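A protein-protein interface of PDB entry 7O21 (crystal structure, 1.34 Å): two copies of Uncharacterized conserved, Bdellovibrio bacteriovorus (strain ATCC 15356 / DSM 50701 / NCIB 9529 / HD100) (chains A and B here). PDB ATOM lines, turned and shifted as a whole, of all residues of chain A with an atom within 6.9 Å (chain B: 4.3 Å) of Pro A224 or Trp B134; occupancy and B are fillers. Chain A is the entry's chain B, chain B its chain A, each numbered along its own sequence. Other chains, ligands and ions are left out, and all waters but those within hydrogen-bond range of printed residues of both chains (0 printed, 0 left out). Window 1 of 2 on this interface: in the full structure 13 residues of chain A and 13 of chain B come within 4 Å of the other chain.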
ATOM      1  N   LEU A 121      -7.412  30.406  11.820  1.00  0.00           N
ATOM      2  CA  LEU A 121      -8.872  30.456  11.824  1.00  0.00           C
ATOM      3  C   LEU A 121      -9.404  31.877  11.956  1.00  0.00           C
ATOM      4  O   LEU A 121     -10.468  32.190  11.396  1.00  0.00           O
ATOM      5  CB  LEU A 121      -9.459  29.519  12.884  1.00  0.00           C
ATOM      6  CG  LEU A 121      -9.405  28.003  12.634  1.00  0.00           C
ATOM      7  CD1 LEU A 121     -10.147  27.251  13.741  1.00  0.00           C
ATOM      8  CD2 LEU A 121      -9.963  27.619  11.264  1.00  0.00           C
ATOM      9  N   PHE A 221     -20.538  30.744  16.202  1.00  0.00           N
ATOM     10  CA  PHE A 221     -19.590  29.673  16.447  1.00  0.00           C
ATOM     11  C   PHE A 221     -19.630  28.632  15.340  1.00  0.00           C
ATOM     12  O   PHE A 221     -20.698  28.285  14.820  1.00  0.00           O
ATOM     13  CB  PHE A 221     -19.958  29.007  17.771  1.00  0.00           C
ATOM     14  CG  PHE A 221     -19.214  27.729  18.044  1.00  0.00           C
ATOM     15  CD1 PHE A 221     -17.977  27.776  18.658  1.00  0.00           C
ATOM     16  CD2 PHE A 221     -19.752  26.495  17.723  1.00  0.00           C
ATOM     17  CE1 PHE A 221     -17.277  26.623  18.934  1.00  0.00           C
ATOM     18  CE2 PHE A 221     -19.056  25.332  17.994  1.00  0.00           C
ATOM     19  CZ  PHE A 221     -17.826  25.388  18.616  1.00  0.00           C
ATOM     20  N   LYS A 222     -18.448  28.119  15.005  1.00  0.00           N
ATOM     21  CA  LYS A 222     -18.297  26.995  14.096  1.00  0.00           C
ATOM     22  C   LYS A 222     -17.218  26.065  14.621  1.00  0.00           C
ATOM     23  O   LYS A 222     -16.250  26.491  15.264  1.00  0.00           O
ATOM     24  CB  LYS A 222     -17.925  27.454  12.671  1.00  0.00           C
ATOM     25  CG  LYS A 222     -18.834  28.524  12.132  1.00  0.00           C
ATOM     26  CD  LYS A 222     -19.802  27.962  11.113  1.00  0.00           C
ATOM     27  CE  LYS A 222     -20.673  29.067  10.520  1.00  0.00           C
ATOM     28  NZ  LYS A 222     -22.072  29.016  11.039  1.00  0.00           N
ATOM     29  N   ALA A 223     -17.415  24.780  14.365  1.00  0.00           N
ATOM     30  CA  ALA A 223     -16.386  23.768  14.534  1.00  0.00           C
ATOM     31  C   ALA A 223     -16.622  22.745  13.445  1.00  0.00           C
ATOM     32  O   ALA A 223     -17.712  22.709  12.862  1.00  0.00           O
ATOM     33  CB  ALA A 223     -16.467  23.094  15.908  1.00  0.00           C
ATOM     34  N   PRO A 224     -15.631  21.922  13.125  1.00  0.00           N
ATOM     35  CA  PRO A 224     -15.865  20.923  12.068  1.00  0.00           C
ATOM     36  C   PRO A 224     -17.108  20.107  12.388  1.00  0.00           C
ATOM     37  O   PRO A 224     -17.155  19.438  13.423  1.00  0.00           O
ATOM     38  CB  PRO A 224     -14.597  20.065  12.097  1.00  0.00           C
ATOM     39  CG  PRO A 224     -13.533  20.995  12.669  1.00  0.00           C
ATOM     40  CD  PRO A 224     -14.267  21.851  13.679  1.00  0.00           C
ATOM     41  N   GLY A 225     -18.131  20.172  11.531  1.00  0.00           N
ATOM     42  CA  GLY A 225     -19.350  19.428  11.764  1.00  0.00           C
ATOM     43  C   GLY A 225     -20.441  20.161  12.516  1.00  0.00           C
ATOM     44  O   GLY A 225     -21.537  19.592  12.682  1.00  0.00           O
ATOM     45  N   PHE A 226     -20.190  21.388  12.990  1.00  0.00           N
ATOM     46  CA  PHE A 226     -21.103  22.035  13.921  1.00  0.00           C
ATOM     47  C   PHE A 226     -21.288  23.515  13.614  1.00  0.00           C
ATOM     48  O   PHE A 226     -20.375  24.195  13.138  1.00  0.00           O
ATOM     49  CB  PHE A 226     -20.550  21.990  15.345  1.00  0.00           C
ATOM     50  CG  PHE A 226     -20.468  20.604  15.933  1.00  0.00           C
ATOM     51  CD1 PHE A 226     -21.593  20.001  16.479  1.00  0.00           C
ATOM     52  CD2 PHE A 226     -19.276  19.903  15.931  1.00  0.00           C
ATOM     53  CE1 PHE A 226     -21.529  18.736  17.029  1.00  0.00           C
ATOM     54  CE2 PHE A 226     -19.192  18.632  16.485  1.00  0.00           C
ATOM     55  CZ  PHE A 226     -20.324  18.044  17.038  1.00  0.00           C
ATOM     56  N   ASN A 227     -22.470  24.014  13.959  1.00  0.00           N
ATOM     57  CA  ASN A 227     -22.717  25.423  14.238  1.00  0.00           C
ATOM     58  C   ASN A 227     -23.147  25.540  15.700  1.00  0.00           C
ATOM     59  O   ASN A 227     -23.161  24.553  16.440  1.00  0.00           O
ATOM     60  CB  ASN A 227     -23.723  26.037  13.258  1.00  0.00           C
ATOM     61  CG  ASN A 227     -25.026  25.267  13.194  1.00  0.00           C
ATOM     62  OD1 ASN A 227     -25.468  24.692  14.181  1.00  0.00           O
ATOM     63  ND2 ASN A 227     -25.642  25.244  12.015  1.00  0.00           N
ATOM     64  N   TRP A 231     -24.027  22.271  17.974  1.00  0.00           N
ATOM     65  CA  TRP A 231     -23.096  22.079  19.084  1.00  0.00           C
ATOM     66  C   TRP A 231     -23.845  21.992  20.411  1.00  0.00           C
ATOM     67  O   TRP A 231     -23.646  21.050  21.190  1.00  0.00           O
ATOM     68  CB  TRP A 231     -22.092  23.237  19.091  1.00  0.00           C
ATOM     69  CG  TRP A 231     -21.015  23.168  20.139  1.00  0.00           C
ATOM     70  CD1 TRP A 231     -21.059  23.695  21.404  1.00  0.00           C
ATOM     71  CD2 TRP A 231     -19.726  22.563  19.997  1.00  0.00           C
ATOM     72  NE1 TRP A 231     -19.880  23.440  22.058  1.00  0.00           N
ATOM     73  CE2 TRP A 231     -19.041  22.751  21.217  1.00  0.00           C
ATOM     74  CE3 TRP A 231     -19.086  21.874  18.962  1.00  0.00           C
ATOM     75  CZ2 TRP A 231     -17.743  22.282  21.426  1.00  0.00           C
ATOM     76  CZ3 TRP A 231     -17.799  21.398  19.172  1.00  0.00           C
ATOM     77  CH2 TRP A 231     -17.138  21.610  20.396  1.00  0.00           C
ATOM     78  N   GLU A 296     -13.778  26.035  18.120  1.00  0.00           N
ATOM     79  CA  GLU A 296     -13.239  25.094  19.099  1.00  0.00           C
ATOM     80  C   GLU A 296     -12.776  23.850  18.357  1.00  0.00           C
ATOM     81  O   GLU A 296     -13.550  23.255  17.597  1.00  0.00           O
ATOM     82  CB  GLU A 296     -14.294  24.761  20.163  1.00  0.00           C
ATOM     83  CG  GLU A 296     -13.836  23.795  21.253  1.00  0.00           C
ATOM     84  CD  GLU A 296     -14.715  23.838  22.490  1.00  0.00           C
ATOM     85  OE1 GLU A 296     -15.495  24.803  22.645  1.00  0.00           O
ATOM     86  OE2 GLU A 296     -14.651  22.896  23.305  1.00  0.00           O
ATOM     87  N   GLU A 297     -11.506  23.489  18.540  1.00  0.00           N
ATOM     88  CA  GLU A 297     -10.884  22.365  17.856  1.00  0.00           C
ATOM     89  C   GLU A 297     -10.436  21.316  18.863  1.00  0.00           C
ATOM     90  O   GLU A 297     -10.028  21.639  19.988  1.00  0.00           O
ATOM     91  CB  GLU A 297      -9.657  22.823  17.067  1.00  0.00           C
ATOM     92  CG  GLU A 297      -9.957  23.829  15.988  1.00  0.00           C
ATOM     93  CD  GLU A 297      -8.708  24.220  15.200  1.00  0.00           C
ATOM     94  OE1 GLU A 297      -7.643  24.457  15.817  1.00  0.00           O
ATOM     95  OE2 GLU A 297      -8.788  24.277  13.959  1.00  0.00           O
ATOM     96  N   TRP A 298     -10.477  20.055  18.436  1.00  0.00           N
ATOM     97  CA  TRP A 298     -10.000  18.929  19.224  1.00  0.00           C
ATOM     98  C   TRP A 298      -9.273  17.977  18.290  1.00  0.00           C
ATOM     99  O   TRP A 298      -9.776  17.671  17.203  1.00  0.00           O
ATOM    100  CB  TRP A 298     -11.166  18.200  19.903  1.00  0.00           C
ATOM    101  CG  TRP A 298     -10.757  17.080  20.818  1.00  0.00           C
ATOM    102  CD1 TRP A 298     -10.493  17.163  22.153  1.00  0.00           C
ATOM    103  CD2 TRP A 298     -10.584  15.701  20.462  1.00  0.00           C
ATOM    104  NE1 TRP A 298     -10.156  15.925  22.649  1.00  0.00           N
ATOM    105  CE2 TRP A 298     -10.206  15.014  21.629  1.00  0.00           C
ATOM    106  CE3 TRP A 298     -10.717  14.984  19.269  1.00  0.00           C
ATOM    107  CZ2 TRP A 298      -9.958  13.642  21.642  1.00  0.00           C
ATOM    108  CZ3 TRP A 298     -10.469  13.620  19.283  1.00  0.00           C
ATOM    109  CH2 TRP A 298     -10.093  12.966  20.461  1.00  0.00           C
ATOM    110  N   LEU B  99     -13.718  10.337  12.808  1.00  0.00           N
ATOM    111  CA  LEU B  99     -14.477  10.862  13.931  1.00  0.00           C
ATOM    112  C   LEU B  99     -15.623   9.915  14.250  1.00  0.00           C
ATOM    113  O   LEU B  99     -16.210   9.295  13.356  1.00  0.00           O
ATOM    114  CB  LEU B  99     -15.077  12.229  13.583  1.00  0.00           C
ATOM    115  CG  LEU B  99     -14.092  13.304  13.136  1.00  0.00           C
ATOM    116  CD1 LEU B  99     -14.821  14.520  12.583  1.00  0.00           C
ATOM    117  CD2 LEU B  99     -13.232  13.689  14.314  1.00  0.00           C
ATOM    118  N   ILE B 104     -18.938  13.399  17.760  1.00  0.00           N
ATOM    119  CA  ILE B 104     -19.913  13.866  16.776  1.00  0.00           C
ATOM    120  C   ILE B 104     -21.258  13.175  16.974  1.00  0.00           C
ATOM    121  O   ILE B 104     -21.307  11.996  17.358  1.00  0.00           O
ATOM    122  CB  ILE B 104     -19.401  13.720  15.333  1.00  0.00           C
ATOM    123  CG1 ILE B 104     -18.993  12.280  15.044  1.00  0.00           C
ATOM    124  CG2 ILE B 104     -18.225  14.659  15.091  1.00  0.00           C
ATOM    125  CD1 ILE B 104     -18.805  12.007  13.547  1.00  0.00           C
ATOM    126  N   TYR B 109     -24.500  12.123  11.800  1.00  0.00           N
ATOM    127  CA  TYR B 109     -23.359  11.512  11.132  1.00  0.00           C
ATOM    128  C   TYR B 109     -23.349   9.998  11.228  1.00  0.00           C
ATOM    129  O   TYR B 109     -22.431   9.362  10.697  1.00  0.00           O
ATOM    130  CB  TYR B 109     -22.048  12.098  11.691  1.00  0.00           C
ATOM    131  CG  TYR B 109     -22.004  13.589  11.491  1.00  0.00           C
ATOM    132  CD1 TYR B 109     -21.995  14.137  10.218  1.00  0.00           C
ATOM    133  CD2 TYR B 109     -22.003  14.458  12.586  1.00  0.00           C
ATOM    134  CE1 TYR B 109     -21.993  15.492  10.030  1.00  0.00           C
ATOM    135  CE2 TYR B 109     -21.993  15.818  12.405  1.00  0.00           C
ATOM    136  CZ  TYR B 109     -21.979  16.329  11.128  1.00  0.00           C
ATOM    137  OH  TYR B 109     -21.982  17.677  10.903  1.00  0.00           O
ATOM    138  N   ALA B 113     -17.488   9.322  10.739  1.00  0.00           N
ATOM    139  CA  ALA B 113     -17.274  10.318   9.699  1.00  0.00           C
ATOM    140  C   ALA B 113     -15.795  10.369   9.385  1.00  0.00           C
ATOM    141  O   ALA B 113     -14.953  10.182  10.265  1.00  0.00           O
ATOM    142  CB  ALA B 113     -17.724  11.726  10.112  1.00  0.00           C
ATOM    143  N   PHE B 114     -15.483  10.644   8.124  1.00  0.00           N
ATOM    144  CA  PHE B 114     -14.117  10.896   7.696  1.00  0.00           C
ATOM    145  C   PHE B 114     -14.068  12.281   7.079  1.00  0.00           C
ATOM    146  O   PHE B 114     -14.875  12.598   6.201  1.00  0.00           O
ATOM    147  CB  PHE B 114     -13.671   9.855   6.674  1.00  0.00           C
ATOM    148  CG  PHE B 114     -13.548   8.479   7.245  1.00  0.00           C
ATOM    149  CD1 PHE B 114     -14.642   7.618   7.243  1.00  0.00           C
ATOM    150  CD2 PHE B 114     -12.349   8.044   7.803  1.00  0.00           C
ATOM    151  CE1 PHE B 114     -14.543   6.351   7.781  1.00  0.00           C
ATOM    152  CE2 PHE B 114     -12.249   6.768   8.350  1.00  0.00           C
ATOM    153  CZ  PHE B 114     -13.350   5.923   8.337  1.00  0.00           C
ATOM    154  N   THR B 115     -13.141  13.110   7.560  1.00  0.00           N
ATOM    155  CA  THR B 115     -13.023  14.447   7.009  1.00  0.00           C
ATOM    156  C   THR B 115     -12.196  14.402   5.732  1.00  0.00           C
ATOM    157  O   THR B 115     -11.457  13.445   5.476  1.00  0.00           O
ATOM    158  CB  THR B 115     -12.347  15.368   8.024  1.00  0.00           C
ATOM    159  OG1 THR B 115     -10.980  14.951   8.200  1.00  0.00           O
ATOM    160  CG2 THR B 115     -13.076  15.313   9.375  1.00  0.00           C
ATOM    161  N   GLY B 132     -17.757  22.542   4.533  1.00  0.00           N
ATOM    162  CA  GLY B 132     -16.840  21.418   4.463  1.00  0.00           C
ATOM    163  C   GLY B 132     -17.476  20.175   3.869  1.00  0.00           C
ATOM    164  O   GLY B 132     -18.699  20.032   3.779  1.00  0.00           O
ATOM    165  N   ILE B 133     -16.611  19.250   3.452  1.00  0.00           N
ATOM    166  CA  ILE B 133     -17.032  17.981   2.869  1.00  0.00           C
ATOM    167  C   ILE B 133     -16.485  16.868   3.743  1.00  0.00           C
ATOM    168  O   ILE B 133     -15.265  16.772   3.940  1.00  0.00           O
ATOM    169  CB  ILE B 133     -16.526  17.809   1.429  1.00  0.00           C
ATOM    170  CG1 ILE B 133     -17.019  18.951   0.542  1.00  0.00           C
ATOM    171  CG2 ILE B 133     -16.961  16.468   0.859  1.00  0.00           C
ATOM    172  CD1 ILE B 133     -16.649  18.777  -0.914  1.00  0.00           C
ATOM    173  N   TRP B 134     -17.383  16.005   4.224  1.00  0.00           N
ATOM    174  CA  TRP B 134     -17.042  14.785   4.931  1.00  0.00           C
ATOM    175  C   TRP B 134     -17.696  13.615   4.213  1.00  0.00           C
ATOM    176  O   TRP B 134     -18.693  13.775   3.500  1.00  0.00           O
ATOM    177  CB  TRP B 134     -17.626  14.785   6.352  1.00  0.00           C
ATOM    178  CG  TRP B 134     -16.995  15.716   7.352  1.00  0.00           C
ATOM    179  CD1 TRP B 134     -15.992  16.611   7.137  1.00  0.00           C
ATOM    180  CD2 TRP B 134     -17.336  15.813   8.738  1.00  0.00           C
ATOM    181  NE1 TRP B 134     -15.694  17.278   8.309  1.00  0.00           N
ATOM    182  CE2 TRP B 134     -16.504  16.798   9.308  1.00  0.00           C
ATOM    183  CE3 TRP B 134     -18.273  15.164   9.553  1.00  0.00           C
ATOM    184  CZ2 TRP B 134     -16.569  17.141  10.662  1.00  0.00           C
ATOM    185  CZ3 TRP B 134     -18.343  15.509  10.891  1.00  0.00           C
ATOM    186  CH2 TRP B 134     -17.491  16.484  11.436  1.00  0.00           C
ATOM    187  N   LEU B 135     -17.149  12.424   4.448  1.00  0.00           N
ATOM    188  CA  LEU B 135     -17.817  11.165   4.137  1.00  0.00           C
ATOM    189  C   LEU B 135     -18.350  10.616   5.458  1.00  0.00           C
ATOM    190  O   LEU B 135     -17.577  10.428   6.402  1.00  0.00           O
ATOM    191  CB  LEU B 135     -16.812  10.185   3.531  1.00  0.00           C
ATOM    192  CG  LEU B 135     -17.231   8.711   3.507  1.00  0.00           C
ATOM    193  CD1 LEU B 135     -18.377   8.408   2.517  1.00  0.00           C
ATOM    194  CD2 LEU B 135     -16.010   7.870   3.177  1.00  0.00           C
ATOM    195  N   HIS B 136     -19.664  10.433   5.564  1.00  0.00           N
ATOM    196  CA  HIS B 136     -20.203  10.020   6.855  1.00  0.00           C
ATOM    197  C   HIS B 136     -21.461   9.190   6.665  1.00  0.00           C
ATOM    198  O   HIS B 136     -21.878   8.906   5.545  1.00  0.00           O
ATOM    199  CB  HIS B 136     -20.430  11.216   7.795  1.00  0.00           C
ATOM    200  CG  HIS B 136     -21.479  12.179   7.335  1.00  0.00           C
ATOM    201  ND1 HIS B 136     -22.834  11.923   7.450  1.00  0.00           N
ATOM    202  CD2 HIS B 136     -21.376  13.423   6.804  1.00  0.00           C
ATOM    203  CE1 HIS B 136     -23.513  12.962   6.994  1.00  0.00           C
ATOM    204  NE2 HIS B 136     -22.651  13.885   6.596  1.00  0.00           N
ATOM    205  N   CYS B 151     -21.851  16.822   1.526  1.00  0.00           N
ATOM    206  CA  CYS B 151     -21.227  15.668   2.154  1.00  0.00           C
ATOM    207  C   CYS B 151     -21.613  14.398   1.416  1.00  0.00           C
ATOM    208  O   CYS B 151     -22.705  14.291   0.854  1.00  0.00           O
ATOM    209  CB  CYS B 151     -21.689  15.557   3.595  1.00  0.00           C
ATOM    210  SG  CYS B 151     -20.785  16.722   4.659  1.00  0.00           S
ATOM    211  N   VAL B 152     -20.716  13.424   1.437  1.00  0.00           N
ATOM    212  CA  VAL B 152     -21.014  12.094   0.904  1.00  0.00           C
ATOM    213  C   VAL B 152     -21.573  11.245   2.037  1.00  0.00           C
ATOM    214  O   VAL B 152     -20.922  11.079   3.074  1.00  0.00           O
ATOM    215  CB  VAL B 152     -19.758  11.444   0.311  1.00  0.00           C
ATOM    216  CG1 VAL B 152     -20.100  10.061  -0.257  1.00  0.00           C
ATOM    217  CG2 VAL B 152     -19.120  12.353  -0.741  1.00  0.00           C
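Hydrophobic or aromatic side chains of chain B within 4 Å of the printed part of chain A: Tyr B109 and Trp B134. Of the 12 printed residues of chain A, 2 touch a printed residue of chain B. Among the printed residues, no Asp or Glu carboxylate lies within 4 Å of a Lys or Arg side-chain nitrogen of the other chain.
N of Trp B134 lies within hydrogen-bond range of SG of Cys B151 (3.5 Å). N of Val B152 lies within hydrogen-bond range of O of Trp B134 (2.9 Å).
OH of Tyr B109 sits at hydrogen-bond distance from O of Gly A225 (2.7 Å).
Pro A224 touches one residue of chain B. Of the printed residues of chain A, Tyr B109 touches Gly A225 (2.7 Å). Of the printed residues of chain B, Gly A225 touches Tyr B109 and Trp B134. Phe A221 touches none of the printed residues of chain B. Leu B135 touches none of the printed residues of chain A. The nearest residue of chain A that does not touch Trp B134 is Phe A226 (5.7 Å).
Pro A224 touches Trp B134. CH2 of Trp B134 touches CA of Gly A225 (3.5 Å).
No position is printed for both chains.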
